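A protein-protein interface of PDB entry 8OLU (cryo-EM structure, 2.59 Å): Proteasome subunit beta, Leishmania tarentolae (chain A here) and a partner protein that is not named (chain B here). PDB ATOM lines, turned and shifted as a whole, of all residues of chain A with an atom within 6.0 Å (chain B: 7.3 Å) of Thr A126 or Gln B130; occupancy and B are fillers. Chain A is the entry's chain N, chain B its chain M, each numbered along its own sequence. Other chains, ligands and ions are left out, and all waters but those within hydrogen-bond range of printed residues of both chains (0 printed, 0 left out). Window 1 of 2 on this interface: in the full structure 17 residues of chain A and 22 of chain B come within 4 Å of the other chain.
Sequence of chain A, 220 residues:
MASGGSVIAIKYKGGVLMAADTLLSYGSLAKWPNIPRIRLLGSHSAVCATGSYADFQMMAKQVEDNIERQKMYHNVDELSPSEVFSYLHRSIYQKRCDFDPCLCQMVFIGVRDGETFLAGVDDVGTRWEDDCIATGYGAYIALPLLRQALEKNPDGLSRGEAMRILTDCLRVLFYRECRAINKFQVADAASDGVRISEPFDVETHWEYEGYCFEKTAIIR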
ATOM      1  N   PHE A  85      -6.251  -7.798 -26.306  1.00  0.00           N
ATOM      2  CA  PHE A  85      -5.114  -7.081 -25.858  1.00  0.00           C
ATOM      3  C   PHE A  85      -5.536  -5.839 -25.141  1.00  0.00           C
ATOM      4  O   PHE A  85      -4.922  -5.500 -24.172  1.00  0.00           O
ATOM      5  CB  PHE A  85      -4.224  -6.649 -26.995  1.00  0.00           C
ATOM      6  CG  PHE A  85      -2.982  -6.019 -26.453  1.00  0.00           C
ATOM      7  CD1 PHE A  85      -2.100  -6.774 -25.719  1.00  0.00           C
ATOM      8  CD2 PHE A  85      -2.752  -4.689 -26.597  1.00  0.00           C
ATOM      9  CE1 PHE A  85      -1.000  -6.213 -25.095  1.00  0.00           C
ATOM     10  CE2 PHE A  85      -1.626  -4.110 -26.058  1.00  0.00           C
ATOM     11  CZ  PHE A  85      -0.766  -4.865 -25.257  1.00  0.00           C
ATOM     12  N   HIS A  89      -4.678  -5.062 -21.266  1.00  0.00           N
ATOM     13  CA  HIS A  89      -3.992  -3.850 -20.919  1.00  0.00           C
ATOM     14  C   HIS A  89      -4.807  -3.034 -19.961  1.00  0.00           C
ATOM     15  O   HIS A  89      -4.293  -2.383 -19.102  1.00  0.00           O
ATOM     16  CB  HIS A  89      -3.677  -3.093 -22.200  1.00  0.00           C
ATOM     17  CG  HIS A  89      -3.474  -1.653 -21.973  1.00  0.00           C
ATOM     18  ND1 HIS A  89      -4.290  -0.696 -22.490  1.00  0.00           N
ATOM     19  CD2 HIS A  89      -2.592  -1.059 -21.119  1.00  0.00           C
ATOM     20  CE1 HIS A  89      -3.891   0.465 -21.946  1.00  0.00           C
ATOM     21  NE2 HIS A  89      -2.832   0.273 -21.120  1.00  0.00           N
ATOM     22  N   GLY A 120       3.045  -5.402 -26.769  1.00  0.00           N
ATOM     23  CA  GLY A 120       3.666  -5.587 -25.501  1.00  0.00           C
ATOM     24  C   GLY A 120       2.934  -4.789 -24.453  1.00  0.00           C
ATOM     25  O   GLY A 120       2.455  -3.758 -24.793  1.00  0.00           O
ATOM     26  N   VAL A 121       2.788  -5.304 -23.248  1.00  0.00           N
ATOM     27  CA  VAL A 121       2.246  -4.505 -22.188  1.00  0.00           C
ATOM     28  C   VAL A 121       3.112  -4.722 -20.990  1.00  0.00           C
ATOM     29  O   VAL A 121       3.721  -5.745 -20.883  1.00  0.00           O
ATOM     30  CB  VAL A 121       0.781  -4.810 -21.861  1.00  0.00           C
ATOM     31  CG1 VAL A 121       0.588  -6.245 -21.495  1.00  0.00           C
ATOM     32  CG2 VAL A 121       0.229  -3.969 -20.740  1.00  0.00           C
ATOM     33  N   ASP A 122       3.235  -3.728 -20.138  1.00  0.00           N
ATOM     34  CA  ASP A 122       4.093  -3.855 -18.988  1.00  0.00           C
ATOM     35  C   ASP A 122       3.381  -3.549 -17.687  1.00  0.00           C
ATOM     36  O   ASP A 122       2.279  -3.064 -17.642  1.00  0.00           O
ATOM     37  CB  ASP A 122       5.310  -3.011 -19.211  1.00  0.00           C
ATOM     38  CG  ASP A 122       5.034  -1.571 -18.865  1.00  0.00           C
ATOM     39  OD1 ASP A 122       3.895  -1.279 -18.365  1.00  0.00           O
ATOM     40  OD2 ASP A 122       6.005  -0.703 -19.055  1.00  0.00           O
ATOM     41  N   ASP A 123       4.020  -3.880 -16.585  1.00  0.00           N
ATOM     42  CA  ASP A 123       3.345  -3.931 -15.297  1.00  0.00           C
ATOM     43  C   ASP A 123       2.530  -2.671 -15.069  1.00  0.00           C
ATOM     44  O   ASP A 123       1.385  -2.760 -14.639  1.00  0.00           O
ATOM     45  CB  ASP A 123       4.323  -4.174 -14.154  1.00  0.00           C
ATOM     46  CG  ASP A 123       5.691  -3.489 -14.330  1.00  0.00           C
ATOM     47  OD1 ASP A 123       6.402  -3.756 -15.402  1.00  0.00           O
ATOM     48  OD2 ASP A 123       6.045  -2.631 -13.437  1.00  0.00           O
ATOM     49  N   VAL A 124       3.079  -1.522 -15.393  1.00  0.00           N
ATOM     50  CA  VAL A 124       2.352  -0.292 -15.176  1.00  0.00           C
ATOM     51  C   VAL A 124       1.303   0.013 -16.222  1.00  0.00           C
ATOM     52  O   VAL A 124       0.593   0.971 -15.995  1.00  0.00           O
ATOM     53  CB  VAL A 124       3.292   0.915 -15.084  1.00  0.00           C
ATOM     54  CG1 VAL A 124       4.256   0.760 -13.914  1.00  0.00           C
ATOM     55  CG2 VAL A 124       4.063   1.142 -16.366  1.00  0.00           C
ATOM     56  N   GLY A 125       1.141  -0.753 -17.294  1.00  0.00           N
ATOM     57  CA  GLY A 125       0.098  -0.456 -18.276  1.00  0.00           C
ATOM     58  C   GLY A 125       0.694   0.271 -19.492  1.00  0.00           C
ATOM     59  O   GLY A 125      -0.001   0.721 -20.400  1.00  0.00           O
ATOM     60  N   THR A 126       2.013   0.378 -19.559  1.00  0.00           N
ATOM     61  CA  THR A 126       2.544   0.769 -20.822  1.00  0.00           C
ATOM     62  C   THR A 126       2.137  -0.243 -21.854  1.00  0.00           C
ATOM     63  O   THR A 126       2.207  -1.402 -21.593  1.00  0.00           O
ATOM     64  CB  THR A 126       4.058   0.882 -20.808  1.00  0.00           C
ATOM     65  OG1 THR A 126       4.530   1.662 -19.711  1.00  0.00           O
ATOM     66  CG2 THR A 126       4.553   1.582 -22.050  1.00  0.00           C
ATOM     67  N   ARG A 127       1.805   0.189 -23.062  1.00  0.00           N
ATOM     68  CA  ARG A 127       1.554  -0.752 -24.131  1.00  0.00           C
ATOM     69  C   ARG A 127       2.069  -0.203 -25.427  1.00  0.00           C
ATOM     70  O   ARG A 127       1.981   0.971 -25.627  1.00  0.00           O
ATOM     71  CB  ARG A 127       0.071  -1.044 -24.314  1.00  0.00           C
ATOM     72  CG  ARG A 127      -0.766   0.184 -24.587  1.00  0.00           C
ATOM     73  CD  ARG A 127      -2.175  -0.114 -25.052  1.00  0.00           C
ATOM     74  NE  ARG A 127      -2.249  -0.387 -26.466  1.00  0.00           N
ATOM     75  CZ  ARG A 127      -3.217  -1.082 -27.070  1.00  0.00           C
ATOM     76  NH1 ARG A 127      -4.242  -1.607 -26.428  1.00  0.00           N
ATOM     77  NH2 ARG A 127      -3.076  -1.320 -28.355  1.00  0.00           N
ATOM     78  N   TRP A 128       2.442  -1.076 -26.329  1.00  0.00           N
ATOM     79  CA  TRP A 128       3.029  -0.669 -27.562  1.00  0.00           C
ATOM     80  C   TRP A 128       2.904  -1.770 -28.547  1.00  0.00           C
ATOM     81  O   TRP A 128       2.851  -2.894 -28.159  1.00  0.00           O
ATOM     82  CB  TRP A 128       4.488  -0.314 -27.375  1.00  0.00           C
ATOM     83  CG  TRP A 128       5.427  -1.401 -26.946  1.00  0.00           C
ATOM     84  CD1 TRP A 128       6.276  -2.082 -27.736  1.00  0.00           C
ATOM     85  CD2 TRP A 128       5.669  -1.884 -25.629  1.00  0.00           C
ATOM     86  NE1 TRP A 128       6.963  -3.005 -27.001  1.00  0.00           N
ATOM     87  CE2 TRP A 128       6.612  -2.899 -25.720  1.00  0.00           C
ATOM     88  CE3 TRP A 128       5.093  -1.618 -24.395  1.00  0.00           C
ATOM     89  CZ2 TRP A 128       7.069  -3.613 -24.629  1.00  0.00           C
ATOM     90  CZ3 TRP A 128       5.541  -2.305 -23.287  1.00  0.00           C
ATOM     91  CH2 TRP A 128       6.536  -3.282 -23.391  1.00  0.00           C
ATOM     92  N   TRP B 126       9.251  -1.221  -6.781  1.00  0.00           N
ATOM     93  CA  TRP B 126       8.146  -1.068  -7.767  1.00  0.00           C
ATOM     94  C   TRP B 126       7.455   0.277  -7.577  1.00  0.00           C
ATOM     95  O   TRP B 126       6.688   0.472  -6.628  1.00  0.00           O
ATOM     96  CB  TRP B 126       7.078  -2.183  -7.704  1.00  0.00           C
ATOM     97  CG  TRP B 126       6.066  -2.073  -8.828  1.00  0.00           C
ATOM     98  CD1 TRP B 126       6.252  -2.464 -10.121  1.00  0.00           C
ATOM     99  CD2 TRP B 126       4.770  -1.433  -8.803  1.00  0.00           C
ATOM    100  NE1 TRP B 126       5.153  -2.147 -10.878  1.00  0.00           N
ATOM    101  CE2 TRP B 126       4.252  -1.473 -10.108  1.00  0.00           C
ATOM    102  CE3 TRP B 126       4.020  -0.775  -7.821  1.00  0.00           C
ATOM    103  CZ2 TRP B 126       3.001  -0.955 -10.442  1.00  0.00           C
ATOM    104  CZ3 TRP B 126       2.790  -0.233  -8.144  1.00  0.00           C
ATOM    105  CH2 TRP B 126       2.271  -0.360  -9.436  1.00  0.00           C
ATOM    106  N   SER B 127       7.688   1.138  -8.582  1.00  0.00           N
ATOM    107  CA  SER B 127       6.953   2.382  -8.771  1.00  0.00           C
ATOM    108  C   SER B 127       5.795   2.138  -9.710  1.00  0.00           C
ATOM    109  O   SER B 127       5.976   1.436 -10.709  1.00  0.00           O
ATOM    110  CB  SER B 127       7.820   3.482  -9.361  1.00  0.00           C
ATOM    111  OG  SER B 127       7.112   4.724  -9.355  1.00  0.00           O
ATOM    112  N   PRO B 128       4.662   2.815  -9.456  1.00  0.00           N
ATOM    113  CA  PRO B 128       3.538   2.924 -10.405  1.00  0.00           C
ATOM    114  C   PRO B 128       3.728   3.979 -11.510  1.00  0.00           C
ATOM    115  O   PRO B 128       2.830   4.201 -12.319  1.00  0.00           O
ATOM    116  CB  PRO B 128       2.371   3.365  -9.515  1.00  0.00           C
ATOM    117  CG  PRO B 128       3.056   4.205  -8.460  1.00  0.00           C
ATOM    118  CD  PRO B 128       4.442   3.597  -8.240  1.00  0.00           C
ATOM    119  N   TYR B 129       4.925   4.589 -11.522  1.00  0.00           N
ATOM    120  CA  TYR B 129       5.255   5.670 -12.403  1.00  0.00           C
ATOM    121  C   TYR B 129       6.519   5.334 -13.168  1.00  0.00           C
ATOM    122  O   TYR B 129       7.480   4.834 -12.606  1.00  0.00           O
ATOM    123  CB  TYR B 129       5.489   6.950 -11.607  1.00  0.00           C
ATOM    124  CG  TYR B 129       4.281   7.556 -10.944  1.00  0.00           C
ATOM    125  CD1 TYR B 129       3.159   7.896 -11.685  1.00  0.00           C
ATOM    126  CD2 TYR B 129       4.267   7.866  -9.596  1.00  0.00           C
ATOM    127  CE1 TYR B 129       2.049   8.494 -11.112  1.00  0.00           C
ATOM    128  CE2 TYR B 129       3.147   8.442  -8.992  1.00  0.00           C
ATOM    129  CZ  TYR B 129       2.042   8.792  -9.760  1.00  0.00           C
ATOM    130  OH  TYR B 129       0.920   9.395  -9.225  1.00  0.00           O
ATOM    131  N   GLN B 130       6.525   5.737 -14.435  1.00  0.00           N
ATOM    132  CA  GLN B 130       7.593   5.493 -15.385  1.00  0.00           C
ATOM    133  C   GLN B 130       7.595   6.702 -16.327  1.00  0.00           C
ATOM    134  O   GLN B 130       6.532   7.155 -16.746  1.00  0.00           O
ATOM    135  CB  GLN B 130       7.232   4.133 -15.993  1.00  0.00           C
ATOM    136  CG  GLN B 130       8.024   3.671 -17.205  1.00  0.00           C
ATOM    137  CD  GLN B 130       7.524   2.309 -17.658  1.00  0.00           C
ATOM    138  OE1 GLN B 130       7.300   1.421 -16.831  1.00  0.00           O
ATOM    139  NE2 GLN B 130       7.323   2.121 -18.964  1.00  0.00           N
ATOM    140  N   ASP B 131       8.750   7.279 -16.651  1.00  0.00           N
ATOM    141  CA  ASP B 131       8.748   8.306 -17.686  1.00  0.00           C
ATOM    142  C   ASP B 131       9.007   7.626 -19.027  1.00  0.00           C
ATOM    143  O   ASP B 131      10.067   7.046 -19.223  1.00  0.00           O
ATOM    144  CB  ASP B 131       9.779   9.422 -17.438  1.00  0.00           C
ATOM    145  CG  ASP B 131       9.646  10.706 -18.297  1.00  0.00           C
ATOM    146  OD1 ASP B 131       8.996  10.684 -19.412  1.00  0.00           O
ATOM    147  OD2 ASP B 131      10.195  11.769 -17.851  1.00  0.00           O
ATOM    148  N   ASN B 132       8.099   7.767 -19.983  1.00  0.00           N
ATOM    149  CA  ASN B 132       8.323   7.160 -21.285  1.00  0.00           C
ATOM    150  C   ASN B 132       8.921   8.161 -22.253  1.00  0.00           C
ATOM    151  O   ASN B 132       9.149   7.881 -23.415  1.00  0.00           O
ATOM    152  CB  ASN B 132       7.079   6.430 -21.778  1.00  0.00           C
ATOM    153  CG  ASN B 132       6.761   5.299 -20.854  1.00  0.00           C
ATOM    154  OD1 ASN B 132       5.828   5.372 -20.062  1.00  0.00           O
ATOM    155  ND2 ASN B 132       7.609   4.287 -20.890  1.00  0.00           N
ATOM    156  N   GLY B 133       9.187   9.340 -21.733  1.00  0.00           N
ATOM    157  CA  GLY B 133       9.907  10.371 -22.473  1.00  0.00           C
ATOM    158  C   GLY B 133       9.142  11.033 -23.630  1.00  0.00           C
ATOM    159  O   GLY B 133       7.911  11.192 -23.632  1.00  0.00           O
ATOM    160  N   LEU B 153       8.752   5.939 -27.981  1.00  0.00           N
ATOM    161  CA  LEU B 153       8.325   5.520 -26.669  1.00  0.00           C
ATOM    162  C   LEU B 153       9.442   4.767 -25.987  1.00  0.00           C
ATOM    163  O   LEU B 153       9.808   3.741 -26.492  1.00  0.00           O
ATOM    164  CB  LEU B 153       7.133   4.598 -26.829  1.00  0.00           C
ATOM    165  CG  LEU B 153       6.636   4.043 -25.504  1.00  0.00           C
ATOM    166  CD1 LEU B 153       5.790   5.095 -24.836  1.00  0.00           C
ATOM    167  CD2 LEU B 153       5.832   2.770 -25.707  1.00  0.00           C
ATOM    168  N   ASN B 154       9.905   5.264 -24.850  1.00  0.00           N
ATOM    169  CA  ASN B 154      11.109   4.761 -24.239  1.00  0.00           C
ATOM    170  C   ASN B 154      10.703   3.901 -23.070  1.00  0.00           C
ATOM    171  O   ASN B 154       9.699   4.177 -22.448  1.00  0.00           O
ATOM    172  CB  ASN B 154      12.047   5.832 -23.626  1.00  0.00           C
ATOM    173  CG  ASN B 154      12.628   6.765 -24.666  1.00  0.00           C
ATOM    174  OD1 ASN B 154      13.586   6.394 -25.338  1.00  0.00           O
ATOM    175  ND2 ASN B 154      12.004   7.919 -24.874  1.00  0.00           N
ATOM    176  N   GLY B 155      11.515   2.891 -22.773  1.00  0.00           N
ATOM    177  CA  GLY B 155      11.402   2.192 -21.513  1.00  0.00           C
ATOM    178  C   GLY B 155      12.565   2.543 -20.590  1.00  0.00           C
ATOM    179  O   GLY B 155      13.138   3.626 -20.676  1.00  0.00           O
ATOM    180  N   ASP B 156      12.908   1.601 -19.712  1.00  0.00           N
ATOM    181  CA  ASP B 156      14.117   1.722 -18.929  1.00  0.00           C
ATOM    182  C   ASP B 156      15.276   1.229 -19.793  1.00  0.00           C
ATOM    183  O   ASP B 156      15.338   0.058 -20.178  1.00  0.00           O
ATOM    184  CB  ASP B 156      13.926   1.048 -17.562  1.00  0.00           C
ATOM    185  CG  ASP B 156      13.041   1.856 -16.603  1.00  0.00           C
ATOM    186  OD1 ASP B 156      13.343   3.065 -16.373  1.00  0.00           O
ATOM    187  OD2 ASP B 156      12.046   1.284 -16.077  1.00  0.00           O
ATOM    188  N   HIS B 160      11.003   1.056 -26.687  1.00  0.00           N
ATOM    189  CA  HIS B 160       9.950   0.108 -26.975  1.00  0.00           C
ATOM    190  C   HIS B 160       9.473   0.206 -28.387  1.00  0.00           C
ATOM    191  O   HIS B 160       9.054  -0.792 -28.953  1.00  0.00           O
ATOM    192  CB  HIS B 160       8.752   0.372 -26.102  1.00  0.00           C
ATOM    193  CG  HIS B 160       8.925   0.009 -24.672  1.00  0.00           C
ATOM    194  ND1 HIS B 160       9.464  -1.158 -24.240  1.00  0.00           N
ATOM    195  CD2 HIS B 160       8.515   0.703 -23.578  1.00  0.00           C
ATOM    196  CE1 HIS B 160       9.423  -1.168 -22.907  1.00  0.00           C
ATOM    197  NE2 HIS B 160       8.817  -0.036 -22.466  1.00  0.00           N
ATOM    198  N   GLY B 181       5.321  12.211 -20.432  1.00  0.00           N
ATOM    199  CA  GLY B 181       5.348  11.548 -19.147  1.00  0.00           C
ATOM    200  C   GLY B 181       5.115  10.088 -19.399  1.00  0.00           C
ATOM    201  O   GLY B 181       5.528   9.612 -20.464  1.00  0.00           O
ATOM    202  N   MET B 182       4.204   9.558 -18.624  1.00  0.00           N
ATOM    203  CA  MET B 182       3.958   8.157 -18.603  1.00  0.00           C
ATOM    204  C   MET B 182       2.970   7.761 -19.654  1.00  0.00           C
ATOM    205  O   MET B 182       1.821   8.106 -19.566  1.00  0.00           O
ATOM    206  CB  MET B 182       3.341   7.830 -17.265  1.00  0.00           C
ATOM    207  CG  MET B 182       3.412   6.391 -16.988  1.00  0.00           C
ATOM    208  SD  MET B 182       2.801   6.084 -15.374  1.00  0.00           S
ATOM    209  CE  MET B 182       2.966   4.307 -15.430  1.00  0.00           C
ATOM    210  N   GLN B 183       3.366   6.939 -20.586  1.00  0.00           N
ATOM    211  CA  GLN B 183       2.432   6.583 -21.621  1.00  0.00           C
ATOM    212  C   GLN B 183       1.183   5.950 -21.065  1.00  0.00           C
ATOM    213  O   GLN B 183       0.107   6.182 -21.548  1.00  0.00           O
ATOM    214  CB  GLN B 183       3.015   5.590 -22.580  1.00  0.00           C
ATOM    215  CG  GLN B 183       2.105   5.331 -23.744  1.00  0.00           C
ATOM    216  CD  GLN B 183       1.990   3.900 -24.120  1.00  0.00           C
ATOM    217  OE1 GLN B 183       2.070   3.025 -23.279  1.00  0.00           O
ATOM    218  NE2 GLN B 183       1.746   3.680 -25.380  1.00  0.00           N
ATOM    219  N   ALA B 184       1.273   5.196 -20.006  1.00  0.00           N
ATOM    220  CA  ALA B 184       0.100   4.538 -19.481  1.00  0.00           C
ATOM    221  C   ALA B 184      -0.936   5.508 -18.983  1.00  0.00           C
ATOM    222  O   ALA B 184      -2.107   5.225 -19.041  1.00  0.00           O
ATOM    223  CB  ALA B 184       0.511   3.664 -18.325  1.00  0.00           C
ATOM    224  N   ASP B 185      -0.485   6.585 -18.399  1.00  0.00           N
ATOM    225  CA  ASP B 185      -1.389   7.535 -17.793  1.00  0.00           C
ATOM    226  C   ASP B 185      -1.936   8.453 -18.833  1.00  0.00           C
ATOM    227  O   ASP B 185      -3.027   8.915 -18.703  1.00  0.00           O
ATOM    228  CB  ASP B 185      -0.691   8.404 -16.738  1.00  0.00           C
ATOM    229  CG  ASP B 185      -0.693   7.728 -15.363  1.00  0.00           C
ATOM    230  OD1 ASP B 185      -1.480   6.724 -15.225  1.00  0.00           O
ATOM    231  OD2 ASP B 185       0.064   8.193 -14.435  1.00  0.00           O
ATOM    232  N   LEU B 187      -2.761   7.287 -21.695  1.00  0.00           N
ATOM    233  CA  LEU B 187      -3.839   6.510 -22.287  1.00  0.00           C
ATOM    234  C   LEU B 187      -5.059   6.561 -21.396  1.00  0.00           C
ATOM    235  O   LEU B 187      -6.170   6.716 -21.890  1.00  0.00           O
ATOM    236  CB  LEU B 187      -3.383   5.109 -22.543  1.00  0.00           C
ATOM    237  CG  LEU B 187      -2.298   5.071 -23.613  1.00  0.00           C
ATOM    238  CD1 LEU B 187      -1.709   3.681 -23.684  1.00  0.00           C
ATOM    239  CD2 LEU B 187      -2.749   5.451 -24.991  1.00  0.00           C
ATOM    240  N   TYR B 231       0.630  11.083 -14.347  1.00  0.00           N
ATOM    241  CA  TYR B 231       1.978  11.557 -14.518  1.00  0.00           C
ATOM    242  C   TYR B 231       2.025  11.899 -15.984  1.00  0.00           C
ATOM    243  O   TYR B 231       2.686  11.290 -16.799  1.00  0.00           O
ATOM    244  CB  TYR B 231       2.968  10.526 -13.999  1.00  0.00           C
ATOM    245  CG  TYR B 231       4.406  10.781 -14.332  1.00  0.00           C
ATOM    246  CD1 TYR B 231       4.896  12.050 -14.536  1.00  0.00           C
ATOM    247  CD2 TYR B 231       5.309   9.741 -14.380  1.00  0.00           C
ATOM    248  CE1 TYR B 231       6.241  12.277 -14.786  1.00  0.00           C
ATOM    249  CE2 TYR B 231       6.655   9.949 -14.638  1.00  0.00           C
ATOM    250  CZ  TYR B 231       7.127  11.226 -14.854  1.00  0.00           C
ATOM    251  OH  TYR B 231       8.465  11.441 -15.093  1.00  0.00           O
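NE1 of Trp B126 is in hydrogen-bond range of OD2 of Asp A123, at 2.8 Å. OD2 of Asp A122 is in hydrogen-bond range of NE2 of Gln B130, 3.1 Å away. The side-chain hydroxyl (OG1) of Thr A126 lies within hydrogen-bond range of the side-chain amide nitrogen (NE2) of Gln B130, at 2.9 Å. The backbone carbonyl oxygen of Arg A127 sits at hydrogen-bond distance from the side-chain amide nitrogen of Gln B183, at 2.7 Å.
The backbone carbonyl oxygen (O) of Asn B154 sits at hydrogen-bond distance from the side-chain amide nitrogen (ND2) of Asn B132, 2.6 Å away. OD1 of Asp A122 sits close to N of Val A124. The side-chain hydroxyl (OG) of Ser B127 sits at hydrogen-bond distance from the backbone NH (N) of Tyr B129 (3.1 Å). NE2 of His A89 is in hydrogen-bond range of O of Gly A125. O of Gly B181 lies within hydrogen-bond range of N of Asn B132 (3.2 Å). N of Gly A120 lies within hydrogen-bond range of O of Trp A128.
O of Ser B127 touches CG1 of Val A124, at 3.7 Å. CG2 of Val A124 touches OE1 of Gln B130, at 3.3 Å. Val A124 touches Met B182. O of Val A124 touches CB of Ala B184, 3.6 Å away. Gly A125 touches Ala B184. Asn B132 touches Thr A126 (OD1 to OG1, 3.9 Å). Thr A126 touches Gln B183 (CG2 to OE1, 3.1 Å). Arg A127 touches Leu B187. Trp A128 touches Leu B153 (CB to CD2, 3.8 Å). Trp A128 touches His B160 (CD1 to O, 3.3 Å).
Thr A126 touches just these residues of chain B: Gln B130 (2.9 Å), Asn B132 (3.9 Å), Gln B183 (3.1 Å) and Ala B184 (3.8 Å). Gln B130 touches just these residues of chain A: Asp A122 (3.1 Å), Val A124 (3.3 Å) and Thr A126 (2.9 Å). Gly A125 touches just one residue of chain B: Ala B184 (3.6 Å). Printed residues of chain B within 4 Å of Val A124: Ser B127 (3.7 Å), Gln B130 (3.3 Å), Met B182 (3.4 Å) and Ala B184 (3.6 Å). Printed residues of chain A within 4 Å of Leu B153: Trp A128. Asp B185 touches none of the printed residues of chain A. Gly B133 touches none of the printed residues of chain A. The nearest residue of chain B that does not touch Thr A126 is Leu B153 (4.1 Å). The nearest residue of chain A that does not touch Gln B130 is Asp A123 (5.4 Å).
Of the 11 printed residues of chain A, 7 touch a printed residue of chain B. Hydrophobic or aromatic side chains of chain A that line the printed part of chain B: Val A124 and Trp A128. Of the 20 printed residues of chain B, 10 touch a printed residue of chain A. Printed residues of chain B that touch a printed residue of chain A: Trp B126, Ser B127, Gln B130, Asn B132, Leu B153, His B160, Met B182, Gln B183, Ala B184 and Leu B187. Along chain B the printed residues that touch a printed residue of chain A span positions 126 to 187. Among the printed residues, 15 pairs touch across the chains. Among the printed residues, no Asp or Glu carboxylate lies within 4 Å of a Lys or Arg side-chain nitrogen of the other chain.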
